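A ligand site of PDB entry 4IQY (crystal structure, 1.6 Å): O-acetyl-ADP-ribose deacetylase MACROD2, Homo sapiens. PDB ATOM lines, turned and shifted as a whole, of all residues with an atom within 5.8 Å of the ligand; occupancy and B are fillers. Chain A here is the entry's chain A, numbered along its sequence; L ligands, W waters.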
ATOM      1  N   GLY A  74       9.539   5.921   6.285  1.00  0.00           N
ATOM      2  CA  GLY A  74       9.727   4.834   7.223  1.00  0.00           C
ATOM      3  C   GLY A  74       8.886   3.614   6.933  1.00  0.00           C
ATOM      4  O   GLY A  74       8.266   3.498   5.874  1.00  0.00           O
ATOM      5  N   ASP A  75       8.864   2.697   7.909  1.00  0.00           N
ATOM      6  CA  ASP A  75       8.107   1.450   7.832  1.00  0.00           C
ATOM      7  C   ASP A  75       6.616   1.708   8.009  1.00  0.00           C
ATOM      8  O   ASP A  75       6.178   2.194   9.057  1.00  0.00           O
ATOM      9  CB  ASP A  75       8.627   0.530   8.945  1.00  0.00           C
ATOM     10  CG  ASP A  75       8.008  -0.847   8.951  1.00  0.00           C
ATOM     11  OD1 ASP A  75       7.089  -1.111   8.150  1.00  0.00           O
ATOM     12  OD2 ASP A  75       8.437  -1.674   9.785  1.00  0.00           O
ATOM     13  N   ILE A  76       5.831   1.388   6.991  1.00  0.00           N
ATOM     14  CA  ILE A  76       4.410   1.691   6.994  1.00  0.00           C
ATOM     15  C   ILE A  76       3.685   0.897   8.083  1.00  0.00           C
ATOM     16  O   ILE A  76       2.630   1.329   8.578  1.00  0.00           O
ATOM     17  CB  ILE A  76       3.783   1.414   5.605  1.00  0.00           C
ATOM     18  CG1 ILE A  76       2.432   2.113   5.460  1.00  0.00           C
ATOM     19  CG2 ILE A  76       3.640  -0.096   5.344  1.00  0.00           C
ATOM     20  CD1 ILE A  76       1.901   2.093   4.042  1.00  0.00           C
ATOM     21  N   THR A  77       4.241  -0.252   8.462  1.00  0.00           N
ATOM     22  CA  THR A  77       3.553  -1.137   9.398  1.00  0.00           C
ATOM     23  C   THR A  77       3.537  -0.624  10.826  1.00  0.00           C
ATOM     24  O   THR A  77       2.805  -1.147  11.672  1.00  0.00           O
ATOM     25  CB  THR A  77       4.137  -2.583   9.357  1.00  0.00           C
ATOM     26  OG1 THR A  77       5.492  -2.566   9.847  1.00  0.00           O
ATOM     27  CG2 THR A  77       4.091  -3.158   7.932  1.00  0.00           C
ATOM     28  N   ALA A  87       0.802  -2.724  -1.292  1.00  0.00           N
ATOM     29  CA  ALA A  87       1.158  -2.988  -2.694  1.00  0.00           C
ATOM     30  C   ALA A  87       1.165  -4.497  -2.931  1.00  0.00           C
ATOM     31  O   ALA A  87       2.217  -5.179  -2.876  1.00  0.00           O
ATOM     32  CB  ALA A  87       2.514  -2.359  -3.015  1.00  0.00           C
ATOM     33  N   ALA A  88      -0.018  -5.037  -3.199  1.00  0.00           N
ATOM     34  CA  ALA A  88      -0.227  -6.476  -3.192  1.00  0.00           C
ATOM     35  C   ALA A  88      -0.018  -7.078  -4.571  1.00  0.00           C
ATOM     36  O   ALA A  88       0.305  -6.383  -5.523  1.00  0.00           O
ATOM     37  CB  ALA A  88      -1.626  -6.790  -2.677  1.00  0.00           C
ATOM     38  N   ASN A  89      -0.237  -8.379  -4.679  1.00  0.00           N
ATOM     39  CA  ASN A  89      -0.328  -8.993  -5.983  1.00  0.00           C
ATOM     40  C   ASN A  89      -1.727  -9.535  -6.196  1.00  0.00           C
ATOM     41  O   ASN A  89      -2.541  -9.518  -5.261  1.00  0.00           O
ATOM     42  CB  ASN A  89       0.711 -10.102  -6.139  1.00  0.00           C
ATOM     43  CG  ASN A  89       0.492 -11.219  -5.160  1.00  0.00           C
ATOM     44  OD1 ASN A  89      -0.379 -12.079  -5.368  1.00  0.00           O
ATOM     45  ND2 ASN A  89       1.267 -11.238  -4.091  1.00  0.00           N
ATOM     46  N   GLY A  94       0.050 -12.511  -0.201  1.00  0.00           N
ATOM     47  CA  GLY A  94       1.319 -12.091   0.382  1.00  0.00           C
ATOM     48  C   GLY A  94       2.457 -12.175  -0.599  1.00  0.00           C
ATOM     49  O   GLY A  94       2.274 -12.447  -1.791  1.00  0.00           O
ATOM     50  N   GLY A  95       3.658 -11.904  -0.107  1.00  0.00           N
ATOM     51  CA  GLY A  95       4.833 -11.919  -0.952  1.00  0.00           C
ATOM     52  C   GLY A  95       6.009 -11.277  -0.268  1.00  0.00           C
ATOM     53  O   GLY A  95       6.270 -11.504   0.922  1.00  0.00           O
ATOM     54  N   GLY A  96       6.730 -10.468  -1.027  1.00  0.00           N
ATOM     55  CA  GLY A  96       7.914  -9.801  -0.516  1.00  0.00           C
ATOM     56  C   GLY A  96       7.652  -8.322  -0.380  1.00  0.00           C
ATOM     57  O   GLY A  96       6.488  -7.914  -0.400  1.00  0.00           O
ATOM     58  N   GLY A  97       8.713  -7.536  -0.226  1.00  0.00           N
ATOM     59  CA  GLY A  97       8.587  -6.096  -0.155  1.00  0.00           C
ATOM     60  C   GLY A  97       7.600  -5.666   0.913  1.00  0.00           C
ATOM     61  O   GLY A  97       7.527  -6.248   2.002  1.00  0.00           O
ATOM     62  N   VAL A  98       6.832  -4.623   0.621  1.00  0.00           N
ATOM     63  CA  VAL A  98       5.930  -4.095   1.633  1.00  0.00           C
ATOM     64  C   VAL A  98       4.801  -5.090   1.970  1.00  0.00           C
ATOM     65  O   VAL A  98       4.382  -5.202   3.118  1.00  0.00           O
ATOM     66  CB  VAL A  98       5.417  -2.698   1.245  1.00  0.00           C
ATOM     67  CG1 VAL A  98       4.489  -2.744   0.033  1.00  0.00           C
ATOM     68  CG2 VAL A  98       4.687  -2.071   2.439  1.00  0.00           C
ATOM     69  N   ASP A  99       4.361  -5.867   0.982  1.00  0.00           N
ATOM     70  CA  ASP A  99       3.373  -6.919   1.173  1.00  0.00           C
ATOM     71  C   ASP A  99       3.848  -7.916   2.236  1.00  0.00           C
ATOM     72  O   ASP A  99       3.122  -8.232   3.189  1.00  0.00           O
ATOM     73  CB  ASP A  99       3.136  -7.587  -0.194  1.00  0.00           C
ATOM     74  CG  ASP A  99       1.914  -8.485  -0.249  1.00  0.00           C
ATOM     75  OD1 ASP A  99       1.075  -8.529   0.684  1.00  0.00           O
ATOM     76  OD2 ASP A  99       1.775  -9.159  -1.301  1.00  0.00           O
ATOM     77  N   GLY A 100       5.060  -8.415   2.082  1.00  0.00           N
ATOM     78  CA  GLY A 100       5.627  -9.326   3.073  1.00  0.00           C
ATOM     79  C   GLY A 100       5.702  -8.728   4.460  1.00  0.00           C
ATOM     80  O   GLY A 100       5.399  -9.398   5.439  1.00  0.00           O
ATOM     81  N   CYS A 101       6.105  -7.451   4.534  1.00  0.00           N
ATOM     82  CA  CYS A 101       6.182  -6.744   5.815  1.00  0.00           C
ATOM     83  C   CYS A 101       4.814  -6.645   6.457  1.00  0.00           C
ATOM     84  O   CYS A 101       4.653  -6.901   7.655  1.00  0.00           O
ATOM     85  CB  CYS A 101       6.759  -5.336   5.624  1.00  0.00           C
ATOM     86  SG  CYS A 101       8.512  -5.279   5.252  1.00  0.00           S
ATOM     87  N   GLY A 143      -0.805  -3.029  -8.127  1.00  0.00           N
ATOM     88  CA  GLY A 143      -0.262  -2.085  -9.077  1.00  0.00           C
ATOM     89  C   GLY A 143       0.035  -2.757 -10.408  1.00  0.00           C
ATOM     90  O   GLY A 143       0.106  -3.978 -10.491  1.00  0.00           O
ATOM     91  N   PRO A 180       2.114   3.349   0.427  1.00  0.00           N
ATOM     92  CA  PRO A 180       3.503   3.095   0.026  1.00  0.00           C
ATOM     93  C   PRO A 180       3.680   3.449  -1.443  1.00  0.00           C
ATOM     94  O   PRO A 180       2.699   3.803  -2.120  1.00  0.00           O
ATOM     95  CB  PRO A 180       3.627   1.584   0.231  1.00  0.00           C
ATOM     96  CG  PRO A 180       2.258   1.073  -0.147  1.00  0.00           C
ATOM     97  CD  PRO A 180       1.276   2.147   0.287  1.00  0.00           C
ATOM     98  N   CYS A 181       4.901   3.356  -1.940  1.00  0.00           N
ATOM     99  CA  CYS A 181       5.175   3.674  -3.333  1.00  0.00           C
ATOM    100  C   CYS A 181       4.825   2.512  -4.264  1.00  0.00           C
ATOM    101  O   CYS A 181       5.705   1.829  -4.803  1.00  0.00           O
ATOM    102  CB  CYS A 181       6.638   4.106  -3.500  1.00  0.00           C
ATOM    103  SG  CYS A 181       7.057   5.631  -2.597  1.00  0.00           S
ATOM    104  N   ILE A 182       3.533   2.316  -4.455  1.00  0.00           N
ATOM    105  CA  ILE A 182       2.993   1.186  -5.222  1.00  0.00           C
ATOM    106  C   ILE A 182       3.655   1.054  -6.588  1.00  0.00           C
ATOM    107  O   ILE A 182       3.854   2.036  -7.299  1.00  0.00           O
ATOM    108  CB  ILE A 182       1.469   1.363  -5.405  1.00  0.00           C
ATOM    109  CG1 ILE A 182       0.770   1.375  -4.046  1.00  0.00           C
ATOM    110  CG2 ILE A 182       0.905   0.256  -6.287  1.00  0.00           C
ATOM    111  CD1 ILE A 182      -0.646   1.943  -4.133  1.00  0.00           C
ATOM    112  N   SER A 183       3.991  -0.188  -6.925  1.00  0.00           N
ATOM    113  CA  SER A 183       4.555  -0.577  -8.231  1.00  0.00           C
ATOM    114  C   SER A 183       6.004  -0.218  -8.476  1.00  0.00           C
ATOM    115  O   SER A 183       6.559  -0.642  -9.483  1.00  0.00           O
ATOM    116  CB  SER A 183       3.700  -0.098  -9.409  1.00  0.00           C
ATOM    117  OG  SER A 183       2.525  -0.887  -9.534  1.00  0.00           O
ATOM    118  N   THR A 184       6.642   0.550  -7.574  1.00  0.00           N
ATOM    119  CA  THR A 184       8.007   1.015  -7.864  1.00  0.00           C
ATOM    120  C   THR A 184       9.095   0.093  -7.344  1.00  0.00           C
ATOM    121  O   THR A 184      10.294   0.365  -7.506  1.00  0.00           O
ATOM    122  CB  THR A 184       8.271   2.415  -7.282  1.00  0.00           C
ATOM    123  OG1 THR A 184       8.243   2.335  -5.853  1.00  0.00           O
ATOM    124  CG2 THR A 184       7.240   3.439  -7.765  1.00  0.00           C
ATOM    125  N   GLY A 185       8.679  -0.994  -6.706  1.00  0.00           N
ATOM    126  CA  GLY A 185       9.622  -2.034  -6.267  1.00  0.00           C
ATOM    127  C   GLY A 185       9.834  -3.084  -7.349  1.00  0.00           C
ATOM    128  O   GLY A 185      10.311  -2.770  -8.438  1.00  0.00           O
ATOM    129  N   ILE A 186       9.508  -4.336  -7.053  1.00  0.00           N
ATOM    130  CA  ILE A 186       9.753  -5.367  -8.061  1.00  0.00           C
ATOM    131  C   ILE A 186       8.841  -5.197  -9.283  1.00  0.00           C
ATOM    132  O   ILE A 186       9.142  -5.714 -10.347  1.00  0.00           O
ATOM    133  CB  ILE A 186       9.701  -6.813  -7.504  1.00  0.00           C
ATOM    134  CG1 ILE A 186       8.293  -7.181  -7.008  1.00  0.00           C
ATOM    135  CG2 ILE A 186      10.720  -7.002  -6.419  1.00  0.00           C
ATOM    136  CD1 ILE A 186       8.159  -8.662  -6.575  1.00  0.00           C
ATOM    137  N   TYR A 187       7.738  -4.471  -9.148  1.00  0.00           N
ATOM    138  CA  TYR A 187       6.895  -4.229 -10.323  1.00  0.00           C
ATOM    139  C   TYR A 187       7.471  -3.183 -11.280  1.00  0.00           C
ATOM    140  O   TYR A 187       6.920  -2.955 -12.358  1.00  0.00           O
ATOM    141  CB  TYR A 187       5.444  -3.907  -9.927  1.00  0.00           C
ATOM    142  CG  TYR A 187       4.604  -5.119  -9.553  1.00  0.00           C
ATOM    143  CD1 TYR A 187       5.145  -6.395  -9.556  1.00  0.00           C
ATOM    144  CD2 TYR A 187       3.249  -4.992  -9.234  1.00  0.00           C
ATOM    145  CE1 TYR A 187       4.391  -7.506  -9.220  1.00  0.00           C
ATOM    146  CE2 TYR A 187       2.477  -6.091  -8.892  1.00  0.00           C
ATOM    147  CZ  TYR A 187       3.056  -7.344  -8.893  1.00  0.00           C
ATOM    148  OH  TYR A 187       2.320  -8.466  -8.563  1.00  0.00           O
ATOM    149  N   GLY A 188       8.570  -2.541 -10.883  1.00  0.00           N
ATOM    150  CA  GLY A 188       9.433  -1.845 -11.842  1.00  0.00           C
ATOM    151  C   GLY A 188       9.014  -0.518 -12.437  1.00  0.00           C
ATOM    152  O   GLY A 188       9.626  -0.040 -13.382  1.00  0.00           O
ATOM    153  N   CYS A 219       3.849   7.415   2.560  1.00  0.00           N
ATOM    154  CA  CYS A 219       4.899   6.717   3.302  1.00  0.00           C
ATOM    155  C   CYS A 219       5.925   6.193   2.301  1.00  0.00           C
ATOM    156  O   CYS A 219       5.727   5.133   1.713  1.00  0.00           O
ATOM    157  CB  CYS A 219       4.289   5.559   4.096  1.00  0.00           C
ATOM    158  SG  CYS A 219       5.424   4.720   5.222  1.00  0.00           S
ATOM    159  N   VAL A 220       6.977   6.959   2.097  1.00  0.00           N
ATOM    160  CA  VAL A 220       8.073   6.522   1.247  1.00  0.00           C
ATOM    161  C   VAL A 220       8.995   5.688   2.135  1.00  0.00           C
ATOM    162  O   VAL A 220       8.984   5.830   3.351  1.00  0.00           O
ATOM    163  CB  VAL A 220       8.824   7.720   0.609  1.00  0.00           C
ATOM    164  CG1 VAL A 220       7.873   8.531  -0.271  1.00  0.00           C
ATOM    165  CG2 VAL A 220       9.433   8.611   1.675  1.00  0.00           C
ATOM    166  N   PHE A 221       9.768   4.800   1.516  1.00  0.00           N
ATOM    167  CA  PHE A 221      10.636   3.897   2.248  1.00  0.00           C
ATOM    168  C   PHE A 221      12.080   4.203   1.895  1.00  0.00           C
ATOM    169  O   PHE A 221      12.928   4.353   2.759  1.00  0.00           O
ATOM    170  CB  PHE A 221      10.302   2.453   1.840  1.00  0.00           C
ATOM    171  CG  PHE A 221      10.848   1.416   2.781  1.00  0.00           C
ATOM    172  CD1 PHE A 221      10.382   1.318   4.087  1.00  0.00           C
ATOM    173  CD2 PHE A 221      11.807   0.501   2.349  1.00  0.00           C
ATOM    174  CE1 PHE A 221      10.871   0.355   4.951  1.00  0.00           C
ATOM    175  CE2 PHE A 221      12.292  -0.479   3.199  1.00  0.00           C
ATOM    176  CZ  PHE A 221      11.827  -0.554   4.512  1.00  0.00           C
ATOM    177  N   LEU A 222      12.344   4.314   0.592  1.00  0.00           N
ATOM    178  CA  LEU A 222      13.702   4.547   0.111  1.00  0.00           C
ATOM    179  C   LEU A 222      14.029   6.027   0.079  1.00  0.00           C
ATOM    180  O   LEU A 222      13.140   6.865  -0.108  1.00  0.00           O
ATOM    181  CB  LEU A 222      13.857   3.958  -1.287  1.00  0.00           C
ATOM    182  CG  LEU A 222      13.588   2.468  -1.356  1.00  0.00           C
ATOM    183  CD1 LEU A 222      13.809   1.945  -2.770  1.00  0.00           C
ATOM    184  CD2 LEU A 222      14.462   1.723  -0.341  1.00  0.00           C
ATOM    185  N   ASP A 225      12.906   7.816  -3.194  1.00  0.00           N
ATOM    186  CA  ASP A 225      11.517   8.253  -3.258  1.00  0.00           C
ATOM    187  C   ASP A 225      11.256   9.458  -2.372  1.00  0.00           C
ATOM    188  O   ASP A 225      10.486  10.322  -2.747  1.00  0.00           O
ATOM    189  CB  ASP A 225      10.584   7.107  -2.889  1.00  0.00           C
ATOM    190  CG  ASP A 225      10.657   5.984  -3.878  1.00  0.00           C
ATOM    191  OD1 ASP A 225      10.433   6.255  -5.076  1.00  0.00           O
ATOM    192  OD2 ASP A 225      10.981   4.846  -3.466  1.00  0.00           O
HETATM  193  N1  LIG L   1       7.071   0.254   4.480  1.00  0.00           N
HETATM  194  C1  LIG L   1       6.859   1.135   3.462  1.00  0.00           C
HETATM  195  N2  LIG L   1       7.286   0.969   2.190  1.00  0.00           N
HETATM  196  C2  LIG L   1       7.950  -0.167   1.987  1.00  0.00           C
HETATM  197  C3  LIG L   1       8.200  -1.092   3.003  1.00  0.00           C
HETATM  198  C4  LIG L   1       7.747  -0.902   4.297  1.00  0.00           C
HETATM  199  N3  LIG L   1       7.953  -1.821   5.371  1.00  0.00           N
HETATM  200  N4  LIG L   1       8.944  -2.188   2.453  1.00  0.00           N
HETATM  201  C5  LIG L   1       9.120  -1.863   1.150  1.00  0.00           C
HETATM  202  N5  LIG L   1       8.550  -0.662   0.857  1.00  0.00           N
HETATM  203  P1  LIG L   1       7.242  -3.544  -3.571  1.00  0.00           P
HETATM  204  P2  LIG L   1       5.544  -3.469  -5.921  1.00  0.00           P
HETATM  205  C6  LIG L   1       8.482   0.043  -0.409  1.00  0.00           C
HETATM  206  O1  LIG L   1       6.939  -4.028  -2.189  1.00  0.00           O
HETATM  207  O2  LIG L   1       4.169  -2.897  -6.025  1.00  0.00           O
HETATM  208  C7  LIG L   1       5.298  -8.115  -3.559  1.00  0.00           C
HETATM  209  O3  LIG L   1       5.998  -9.314  -3.588  1.00  0.00           O
HETATM  210  C8  LIG L   1       9.551  -0.243  -1.398  1.00  0.00           C
HETATM  211  O4  LIG L   1      10.754   0.355  -1.085  1.00  0.00           O
HETATM  212  O5  LIG L   1       8.303  -4.367  -4.239  1.00  0.00           O
HETATM  213  O6  LIG L   1       6.603  -2.833  -6.729  1.00  0.00           O
HETATM  214  C9  LIG L   1       3.847  -8.326  -3.842  1.00  0.00           C
HETATM  215  O7  LIG L   1       3.345  -9.541  -3.385  1.00  0.00           O
HETATM  216  C10 LIG L   1       8.922   0.338  -2.600  1.00  0.00           C
HETATM  217  O8  LIG L   1       9.121   1.710  -2.652  1.00  0.00           O
HETATM  218  O9  LIG L   1       5.880  -3.534  -4.375  1.00  0.00           O
HETATM  219  C11 LIG L   1       3.768  -8.155  -5.303  1.00  0.00           C
HETATM  220  O10 LIG L   1       3.897  -9.387  -5.921  1.00  0.00           O
HETATM  221  C12 LIG L   1       7.472   0.043  -2.367  1.00  0.00           C
HETATM  222  O11 LIG L   1       7.307  -0.388  -1.039  1.00  0.00           O
HETATM  223  C13 LIG L   1       4.910  -7.242  -5.638  1.00  0.00           C
HETATM  224  O12 LIG L   1       5.779  -7.247  -4.532  1.00  0.00           O
HETATM  225  C14 LIG L   1       6.880  -0.988  -3.325  1.00  0.00           C
HETATM  226  O13 LIG L   1       7.762  -2.065  -3.560  1.00  0.00           O
HETATM  227  C15 LIG L   1       4.413  -5.822  -5.878  1.00  0.00           C
HETATM  228  O14 LIG L   1       5.473  -5.009  -6.324  1.00  0.00           O
HETATM  229  O   HOH W   1      10.686   2.571  -4.666  1.00  0.00           O
HETATM  230  O   HOH W   2       8.504  -7.129  -3.493  1.00  0.00           O
HETATM  231  O   HOH W   3      10.847  -4.015   3.492  1.00  0.00           O
HETATM  232  O   HOH W   4      10.163   4.020  -1.180  1.00  0.00           O
HETATM  233  O   HOH W   5       3.363 -10.741  -8.310  1.00  0.00           O
HETATM  234  O   HOH W   6       6.818   3.085   0.191  1.00  0.00           O
HETATM  235  O   HOH W   7       1.312  -3.759  -6.220  1.00  0.00           O
HETATM  236  O   HOH W   8      12.788  -1.572  -0.883  1.00  0.00           O
HETATM  237  O   HOH W   9      11.129  -3.679  -0.706  1.00  0.00           O
HETATM  238  O   HOH W  10       4.707  -5.539  -1.886  1.00  0.00           O
HETATM  239  O   HOH W  11      10.825  -4.223  -3.437  1.00  0.00           O
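Water W1 lies within hydrogen-bond range of the side-chain carboxylate of Asp 225 (2.6 Å), an oxygen (O8) of the ligand (2.7 Å) and the side-chain hydroxyl of Thr 184 (2.7 Å).
Water W10 lies within hydrogen-bond range of O of Ala 87 (2.7 Å), O1 of the ligand (2.7 Å), N of Asp 99 (2.9 Å), O of Gly 96 (3.3 Å) and N of Val 98 (3.4 Å).
Water W3 bridges a nitrogen (N4) of the ligand (2.8 Å) and the side-chain sulfur of Cys 101 (3.2 Å).
Water W2 bridges O5 of the ligand (2.9 Å) and N of Gly 97 (3.3 Å).
Water W6 lies within hydrogen-bond range of O of Cys 219, N of Cys 181 and N2 of the ligand.
Water W7 lies within hydrogen-bond range of the backbone carbonyl oxygen of Ala 88 (2.9 Å), the backbone NH of Gly 143 (2.9 Å) and an oxygen (O2) of the ligand (3.0 Å).
The side-chain carboxylate (OD2) of Asp 99 lies within hydrogen-bond range of an oxygen (O7) of the ligand (2.6 Å).
An oxygen (O6) of the ligand lies within hydrogen-bond range of the backbone NH (N) of Gly 185 (2.8 Å).
The side-chain amide nitrogen of Asn 89 sits at hydrogen-bond distance from an oxygen (O7) of the ligand, 2.8 Å away.
An oxygen (O2) of the ligand is in hydrogen-bond range of the backbone NH (N) of Ser 183, 2.9 Å away.
N of Val 98 lies within hydrogen-bond range of O1 of the ligand.
The backbone NH of Gly 96 is in hydrogen-bond range of an oxygen (O3) of the ligand, 2.9 Å away.
A nitrogen (N3) of the ligand lies within hydrogen-bond range of the side-chain carboxylate of Asp 75 (3.0 Å).
N1 of the ligand sits at hydrogen-bond distance from N of Ile 76 (3.0 Å).
N of Ile 186 sits at hydrogen-bond distance from O5 of the ligand (3.1 Å).
An oxygen (O6) of the ligand lies within hydrogen-bond range of the backbone NH (N) of Tyr 187, at 3.1 Å.
An oxygen (O10) of the ligand is in hydrogen-bond range of the side-chain hydroxyl of Tyr 187 (3.2 Å).
N of Thr 184 lies within hydrogen-bond range of O6 of the ligand, at 3.5 Å.
OG1 of Thr 184 is in hydrogen-bond range of O8 of the ligand, at 3.4 Å.
O of Gly 94 is in hydrogen-bond range of O7 of the ligand (3.5 Å).
The side-chain sulfur (SG) of Cys 101 is in hydrogen-bond range of a nitrogen (N3) of the ligand, 3.5 Å away.
The side-chain amide nitrogen (ND2) of Asn 89 lies within hydrogen-bond range of the backbone carbonyl oxygen (O) of Gly 94 (2.8 Å).
The backbone NH of Gly 188 sits at hydrogen-bond distance from the backbone carbonyl oxygen of Ser 183, at 3.1 Å.
OD1 of Asp 75 sits at hydrogen-bond distance from OG1 of Thr 77 (2.7 Å).
N of Ile 76 lies close to SG of Cys 219.
SG of Cys 101 sits at hydrogen-bond distance from O of Gly 97 (3.5 Å).
OG1 of Thr 184 sits at hydrogen-bond distance from O of Cys 181, 2.8 Å away.
O of Gly 74 is in hydrogen-bond range of SG of Cys 219 (3.2 Å).
N of Gly 74 sits at hydrogen-bond distance from O of Val 220 (3.0 Å).
O of Gly 74 touches C1 of the ligand (3.7 Å).
CB of Ala 87 touches O2 of the ligand, at 3.5 Å.
O of Ala 88 touches C11 of the ligand, 3.9 Å away.
Gly 95 touches the ligand (CA to O7, 3.7 Å).
Gly 97 touches the ligand (CA to O1, 3.3 Å).
Cys 181 touches the ligand (O to C14, 3.4 Å).
Phe 221 touches the ligand.
Leu 222 touches the ligand (CG to O4, 3.5 Å).
Asp 225 touches the ligand.
Hydrophobic or aromatic side chains within 4 Å of the ligand: Ile 76, Ala 87, Val 98, Ile 186, Tyr 187, Phe 221 and Leu 222.
Along chain A the residues within 4 Å of the ligand span positions 74 to 225.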
